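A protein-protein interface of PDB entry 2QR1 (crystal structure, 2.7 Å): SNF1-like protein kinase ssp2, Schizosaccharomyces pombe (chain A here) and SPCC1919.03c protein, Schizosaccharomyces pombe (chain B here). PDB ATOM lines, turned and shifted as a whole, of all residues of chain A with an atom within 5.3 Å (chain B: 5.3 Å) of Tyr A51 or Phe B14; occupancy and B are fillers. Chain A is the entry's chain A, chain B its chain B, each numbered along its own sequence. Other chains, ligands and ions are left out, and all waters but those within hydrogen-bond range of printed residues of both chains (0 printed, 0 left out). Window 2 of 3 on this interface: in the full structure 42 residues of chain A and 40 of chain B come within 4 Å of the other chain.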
ATOM      1  N   PRO A  44     -22.505  30.525 -26.267  1.00  0.00           N
ATOM      2  CA  PRO A  44     -22.788  30.278 -24.847  1.00  0.00           C
ATOM      3  C   PRO A  44     -21.597  29.735 -24.072  1.00  0.00           C
ATOM      4  O   PRO A  44     -20.738  29.050 -24.637  1.00  0.00           O
ATOM      5  CB  PRO A  44     -23.897  29.218 -24.875  1.00  0.00           C
ATOM      6  CG  PRO A  44     -24.431  29.228 -26.265  1.00  0.00           C
ATOM      7  CD  PRO A  44     -23.303  29.652 -27.149  1.00  0.00           C
ATOM      8  N   LYS A  45     -21.571  30.060 -22.783  1.00  0.00           N
ATOM      9  CA  LYS A  45     -20.621  29.499 -21.835  1.00  0.00           C
ATOM     10  C   LYS A  45     -21.354  29.097 -20.533  1.00  0.00           C
ATOM     11  O   LYS A  45     -21.864  29.967 -19.822  1.00  0.00           O
ATOM     12  CB  LYS A  45     -19.474  30.494 -21.569  1.00  0.00           C
ATOM     13  CG  LYS A  45     -18.671  30.241 -20.265  1.00  0.00           C
ATOM     14  CD  LYS A  45     -18.181  28.790 -20.131  1.00  0.00           C
ATOM     15  CE  LYS A  45     -16.907  28.512 -20.930  1.00  0.00           C
ATOM     16  NZ  LYS A  45     -15.664  28.631 -20.022  1.00  0.00           N
ATOM     17  N   PRO A  46     -21.394  27.784 -20.210  1.00  0.00           N
ATOM     18  CA  PRO A  46     -22.203  27.303 -19.092  1.00  0.00           C
ATOM     19  C   PRO A  46     -21.644  27.668 -17.701  1.00  0.00           C
ATOM     20  O   PRO A  46     -20.466  28.021 -17.585  1.00  0.00           O
ATOM     21  CB  PRO A  46     -22.200  25.787 -19.306  1.00  0.00           C
ATOM     22  CG  PRO A  46     -20.952  25.500 -20.009  1.00  0.00           C
ATOM     23  CD  PRO A  46     -20.681  26.679 -20.881  1.00  0.00           C
ATOM     24  N   VAL A  47     -22.493  27.582 -16.667  1.00  0.00           N
ATOM     25  CA  VAL A  47     -22.090  27.824 -15.263  1.00  0.00           C
ATOM     26  C   VAL A  47     -21.600  26.543 -14.543  1.00  0.00           C
ATOM     27  O   VAL A  47     -22.328  25.932 -13.735  1.00  0.00           O
ATOM     28  CB  VAL A  47     -23.201  28.563 -14.429  1.00  0.00           C
ATOM     29  CG1 VAL A  47     -24.584  27.817 -14.466  1.00  0.00           C
ATOM     30  CG2 VAL A  47     -22.663  28.869 -12.937  1.00  0.00           C
ATOM     31  N   GLY A  49     -21.806  23.631 -15.085  1.00  0.00           N
ATOM     32  CA  GLY A  49     -22.603  22.637 -15.813  1.00  0.00           C
ATOM     33  C   GLY A  49     -22.624  22.816 -17.325  1.00  0.00           C
ATOM     34  O   GLY A  49     -21.650  22.442 -17.976  1.00  0.00           O
ATOM     35  N   LYS A  50     -23.679  23.375 -17.936  1.00  0.00           N
ATOM     36  CA  LYS A  50     -24.924  23.977 -17.376  1.00  0.00           C
ATOM     37  C   LYS A  50     -25.247  25.313 -18.075  1.00  0.00           C
ATOM     38  O   LYS A  50     -24.723  26.376 -17.716  1.00  0.00           O
ATOM     39  CB  LYS A  50     -24.951  24.127 -15.852  1.00  0.00           C
ATOM     40  CG  LYS A  50     -25.998  23.232 -15.186  1.00  0.00           C
ATOM     41  CD  LYS A  50     -25.602  22.817 -13.758  1.00  0.00           C
ATOM     42  CE  LYS A  50     -26.557  21.772 -13.206  1.00  0.00           C
ATOM     43  NZ  LYS A  50     -26.347  21.548 -11.756  1.00  0.00           N
ATOM     44  N   TYR A  51     -26.113  25.257 -19.080  1.00  0.00           N
ATOM     45  CA  TYR A  51     -26.321  26.425 -19.933  1.00  0.00           C
ATOM     46  C   TYR A  51     -27.249  27.507 -19.372  1.00  0.00           C
ATOM     47  O   TYR A  51     -28.348  27.228 -18.876  1.00  0.00           O
ATOM     48  CB  TYR A  51     -26.660  26.017 -21.375  1.00  0.00           C
ATOM     49  CG  TYR A  51     -25.430  25.558 -22.125  1.00  0.00           C
ATOM     50  CD1 TYR A  51     -25.143  24.192 -22.271  1.00  0.00           C
ATOM     51  CD2 TYR A  51     -24.526  26.489 -22.644  1.00  0.00           C
ATOM     52  CE1 TYR A  51     -23.995  23.768 -22.944  1.00  0.00           C
ATOM     53  CE2 TYR A  51     -23.376  26.077 -23.313  1.00  0.00           C
ATOM     54  CZ  TYR A  51     -23.117  24.719 -23.459  1.00  0.00           C
ATOM     55  OH  TYR A  51     -21.979  24.325 -24.123  1.00  0.00           O
ATOM     56  N   ARG A  52     -26.756  28.742 -19.450  1.00  0.00           N
ATOM     57  CA  ARG A  52     -27.411  29.920 -18.894  1.00  0.00           C
ATOM     58  C   ARG A  52     -28.313  30.593 -19.922  1.00  0.00           C
ATOM     59  O   ARG A  52     -27.927  30.803 -21.082  1.00  0.00           O
ATOM     60  CB  ARG A  52     -26.371  30.918 -18.339  1.00  0.00           C
ATOM     61  CG  ARG A  52     -25.195  31.314 -19.297  1.00  0.00           C
ATOM     62  CD  ARG A  52     -24.161  32.238 -18.590  1.00  0.00           C
ATOM     63  NE  ARG A  52     -22.840  32.225 -19.231  1.00  0.00           N
ATOM     64  CZ  ARG A  52     -22.352  33.180 -20.028  1.00  0.00           C
ATOM     65  NH1 ARG A  52     -23.055  34.273 -20.310  1.00  0.00           N
ATOM     66  NH2 ARG A  52     -21.138  33.038 -20.547  1.00  0.00           N
ATOM     67  N   SER A  53     -29.516  30.935 -19.471  1.00  0.00           N
ATOM     68  CA  SER A  53     -30.553  31.525 -20.309  1.00  0.00           C
ATOM     69  C   SER A  53     -30.092  32.634 -21.258  1.00  0.00           C
ATOM     70  O   SER A  53     -30.776  32.939 -22.229  1.00  0.00           O
ATOM     71  CB  SER A  53     -31.659  32.051 -19.409  1.00  0.00           C
ATOM     72  OG  SER A  53     -32.273  33.157 -20.018  1.00  0.00           O
ATOM     73  N   MET A  55     -27.841  32.528 -23.265  1.00  0.00           N
ATOM     74  CA  MET A  55     -27.376  31.949 -24.513  1.00  0.00           C
ATOM     75  C   MET A  55     -28.174  32.482 -25.712  1.00  0.00           C
ATOM     76  O   MET A  55     -27.660  32.518 -26.820  1.00  0.00           O
ATOM     77  CB  MET A  55     -27.331  30.407 -24.448  1.00  0.00           C
ATOM     78  CG  MET A  55     -28.627  29.644 -24.692  1.00  0.00           C
ATOM     79  SD  MET A  55     -28.352  27.842 -24.555  1.00  0.00           S
ATOM     80  CE  MET A  55     -30.051  27.254 -24.548  1.00  0.00           C
ATOM     81  N   PRO B  12     -21.643  26.443 -32.294  1.00  0.00           N
ATOM     82  CA  PRO B  12     -21.370  25.711 -31.047  1.00  0.00           C
ATOM     83  C   PRO B  12     -21.727  24.245 -31.216  1.00  0.00           C
ATOM     84  O   PRO B  12     -22.790  23.926 -31.771  1.00  0.00           O
ATOM     85  CB  PRO B  12     -22.285  26.376 -30.019  1.00  0.00           C
ATOM     86  CG  PRO B  12     -22.549  27.725 -30.564  1.00  0.00           C
ATOM     87  CD  PRO B  12     -22.562  27.576 -32.076  1.00  0.00           C
ATOM     88  N   ALA B  13     -20.828  23.372 -30.763  1.00  0.00           N
ATOM     89  CA  ALA B  13     -20.931  21.946 -31.037  1.00  0.00           C
ATOM     90  C   ALA B  13     -22.192  21.300 -30.463  1.00  0.00           C
ATOM     91  O   ALA B  13     -22.851  20.521 -31.152  1.00  0.00           O
ATOM     92  CB  ALA B  13     -19.684  21.220 -30.559  1.00  0.00           C
ATOM     93  N   PHE B  14     -22.541  21.651 -29.227  1.00  0.00           N
ATOM     94  CA  PHE B  14     -23.623  20.984 -28.507  1.00  0.00           C
ATOM     95  C   PHE B  14     -24.966  21.086 -29.217  1.00  0.00           C
ATOM     96  O   PHE B  14     -25.841  20.238 -29.030  1.00  0.00           O
ATOM     97  CB  PHE B  14     -23.728  21.495 -27.067  1.00  0.00           C
ATOM     98  CG  PHE B  14     -24.287  22.875 -26.954  1.00  0.00           C
ATOM     99  CD1 PHE B  14     -23.446  23.984 -26.994  1.00  0.00           C
ATOM    100  CD2 PHE B  14     -25.657  23.074 -26.807  1.00  0.00           C
ATOM    101  CE1 PHE B  14     -23.961  25.274 -26.899  1.00  0.00           C
ATOM    102  CE2 PHE B  14     -26.186  24.360 -26.708  1.00  0.00           C
ATOM    103  CZ  PHE B  14     -25.336  25.464 -26.755  1.00  0.00           C
ATOM    104  N   LEU B  15     -25.116  22.130 -30.028  1.00  0.00           N
ATOM    105  CA  LEU B  15     -26.261  22.266 -30.921  1.00  0.00           C
ATOM    106  C   LEU B  15     -26.079  21.389 -32.169  1.00  0.00           C
ATOM    107  O   LEU B  15     -26.326  21.830 -33.291  1.00  0.00           O
ATOM    108  CB  LEU B  15     -26.463  23.731 -31.313  1.00  0.00           C
ATOM    109  CG  LEU B  15     -26.553  24.774 -30.189  1.00  0.00           C
ATOM    110  CD1 LEU B  15     -25.963  26.112 -30.602  1.00  0.00           C
ATOM    111  CD2 LEU B  15     -27.979  24.953 -29.711  1.00  0.00           C
ATOM    112  N   THR B  16     -25.608  20.155 -31.952  1.00  0.00           N
ATOM    113  CA  THR B  16     -25.603  19.091 -32.963  1.00  0.00           C
ATOM    114  C   THR B  16     -25.539  17.699 -32.306  1.00  0.00           C
ATOM    115  O   THR B  16     -25.420  16.688 -33.001  1.00  0.00           O
ATOM    116  CB  THR B  16     -24.531  19.311 -34.066  1.00  0.00           C
ATOM    117  OG1 THR B  16     -24.151  20.689 -34.130  1.00  0.00           O
ATOM    118  CG2 THR B  16     -25.069  18.865 -35.420  1.00  0.00           C
ATOM    119  N   SER B  17     -25.679  17.641 -30.983  1.00  0.00           N
ATOM    120  CA  SER B  17     -25.425  16.415 -30.212  1.00  0.00           C
ATOM    121  C   SER B  17     -25.964  15.105 -30.814  1.00  0.00           C
ATOM    122  O   SER B  17     -25.201  14.298 -31.343  1.00  0.00           O
ATOM    123  CB  SER B  17     -25.916  16.575 -28.773  1.00  0.00           C
ATOM    124  OG  SER B  17     -24.874  17.024 -27.925  1.00  0.00           O
ATOM    125  N   THR B  19     -30.604  16.235 -30.648  1.00  0.00           N
ATOM    126  CA  THR B  19     -30.416  17.490 -29.917  1.00  0.00           C
ATOM    127  C   THR B  19     -31.653  17.600 -29.025  1.00  0.00           C
ATOM    128  O   THR B  19     -31.803  18.541 -28.248  1.00  0.00           O
ATOM    129  CB  THR B  19     -30.387  18.751 -30.834  1.00  0.00           C
ATOM    130  OG1 THR B  19     -29.917  18.416 -32.147  1.00  0.00           O
ATOM    131  CG2 THR B  19     -29.506  19.861 -30.228  1.00  0.00           C
ATOM    132  N   GLU B  22     -32.373  16.507 -23.912  1.00  0.00           N
ATOM    133  CA  GLU B  22     -31.003  16.958 -24.124  1.00  0.00           C
ATOM    134  C   GLU B  22     -30.708  18.222 -23.322  1.00  0.00           C
ATOM    135  O   GLU B  22     -31.164  19.310 -23.671  1.00  0.00           O
ATOM    136  CB  GLU B  22     -30.744  17.207 -25.610  1.00  0.00           C
ATOM    137  CG  GLU B  22     -29.599  18.166 -25.890  1.00  0.00           C
ATOM    138  CD  GLU B  22     -28.242  17.495 -25.807  1.00  0.00           C
ATOM    139  OE1 GLU B  22     -28.199  16.263 -25.603  1.00  0.00           O
ATOM    140  OE2 GLU B  22     -27.220  18.198 -25.947  1.00  0.00           O
ATOM    141  N   LEU B  23     -29.943  18.070 -22.246  1.00  0.00           N
ATOM    142  CA  LEU B  23     -29.699  19.166 -21.317  1.00  0.00           C
ATOM    143  C   LEU B  23     -31.076  19.467 -20.734  1.00  0.00           C
ATOM    144  O   LEU B  23     -31.251  19.494 -19.516  1.00  0.00           O
ATOM    145  CB  LEU B  23     -28.467  19.966 -21.744  1.00  0.00           C
ATOM    146  CG  LEU B  23     -27.280  19.951 -20.778  1.00  0.00           C
ATOM    147  CD1 LEU B  23     -26.944  18.527 -20.362  1.00  0.00           C
ATOM    148  CD2 LEU B  23     -26.072  20.632 -21.401  1.00  0.00           C
ATOM    149  N   LEU B  25     -32.459  22.362 -21.838  1.00  0.00           N
ATOM    150  CA  LEU B  25     -31.854  23.672 -21.647  1.00  0.00           C
ATOM    151  C   LEU B  25     -32.849  24.746 -21.273  1.00  0.00           C
ATOM    152  O   LEU B  25     -34.061  24.521 -21.339  1.00  0.00           O
ATOM    153  CB  LEU B  25     -31.080  24.081 -22.900  1.00  0.00           C
ATOM    154  CG  LEU B  25     -30.044  23.095 -23.422  1.00  0.00           C
ATOM    155  CD1 LEU B  25     -30.620  22.334 -24.589  1.00  0.00           C
ATOM    156  CD2 LEU B  25     -28.801  23.821 -23.849  1.00  0.00           C
ATOM    157  N   PRO B  26     -32.338  25.930 -20.886  1.00  0.00           N
ATOM    158  CA  PRO B  26     -33.175  27.022 -20.404  1.00  0.00           C
ATOM    159  C   PRO B  26     -34.028  27.602 -21.520  1.00  0.00           C
ATOM    160  O   PRO B  26     -33.691  27.456 -22.701  1.00  0.00           O
ATOM    161  CB  PRO B  26     -32.149  28.058 -19.952  1.00  0.00           C
ATOM    162  CG  PRO B  26     -30.972  27.805 -20.844  1.00  0.00           C
ATOM    163  CD  PRO B  26     -30.915  26.316 -20.910  1.00  0.00           C
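O of Lys A45 is in hydrogen-bond range of NE of Arg A52 (2.5 Å).
Among the printed residues, merely in contact across the chains: Pro A44 with Pro B12, Pro A44 with Phe B14, Tyr A51 with Phe B14, Tyr A51 with Leu B23, Tyr A51 with Leu B25, Tyr A51 with Pro B26, Arg A52 with Pro B26, Ser A53 with Pro B26, Met A55 with Leu B25 and Met A55 with Pro B26.
Of chain B, only Phe B14 (3.2 Å), Leu B23 (3.8 Å), Leu B25 (3.9 Å) and Pro B26 (3.3 Å) come within 4 Å of Tyr A51. Printed residues of chain B within 4 Å of Ser A53: Pro B26 (3.7 Å). Of the printed residues of chain A, Pro B12 touches Pro A44 (3.99 Å). Phe B14 touches just these residues of chain A: Pro A44 and Tyr A51. Thr B19 touches none of the printed residues of chain A. Of the printed residues of chain A, Leu B25 touches Tyr A51 (3.9 Å) and Met A55 (3.7 Å). The nearest printed residue of chain B that does not touch Tyr A51 is Pro B12 (6.3 Å).
Of the 11 printed residues of chain B, 5 touch a printed residue of chain A. Of the 10 printed residues of chain A, 5 touch a printed residue of chain B. Printed residues of chain A that touch a printed residue of chain B: Pro A44, Tyr A51, Arg A52, Ser A53 and Met A55. Along chain A the printed residues that touch a printed residue of chain B span positions 44 to 55. Among the printed residues, no Asp or Glu carboxylate lies within 4 Å of a Lys or Arg side-chain nitrogen of the other chain.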
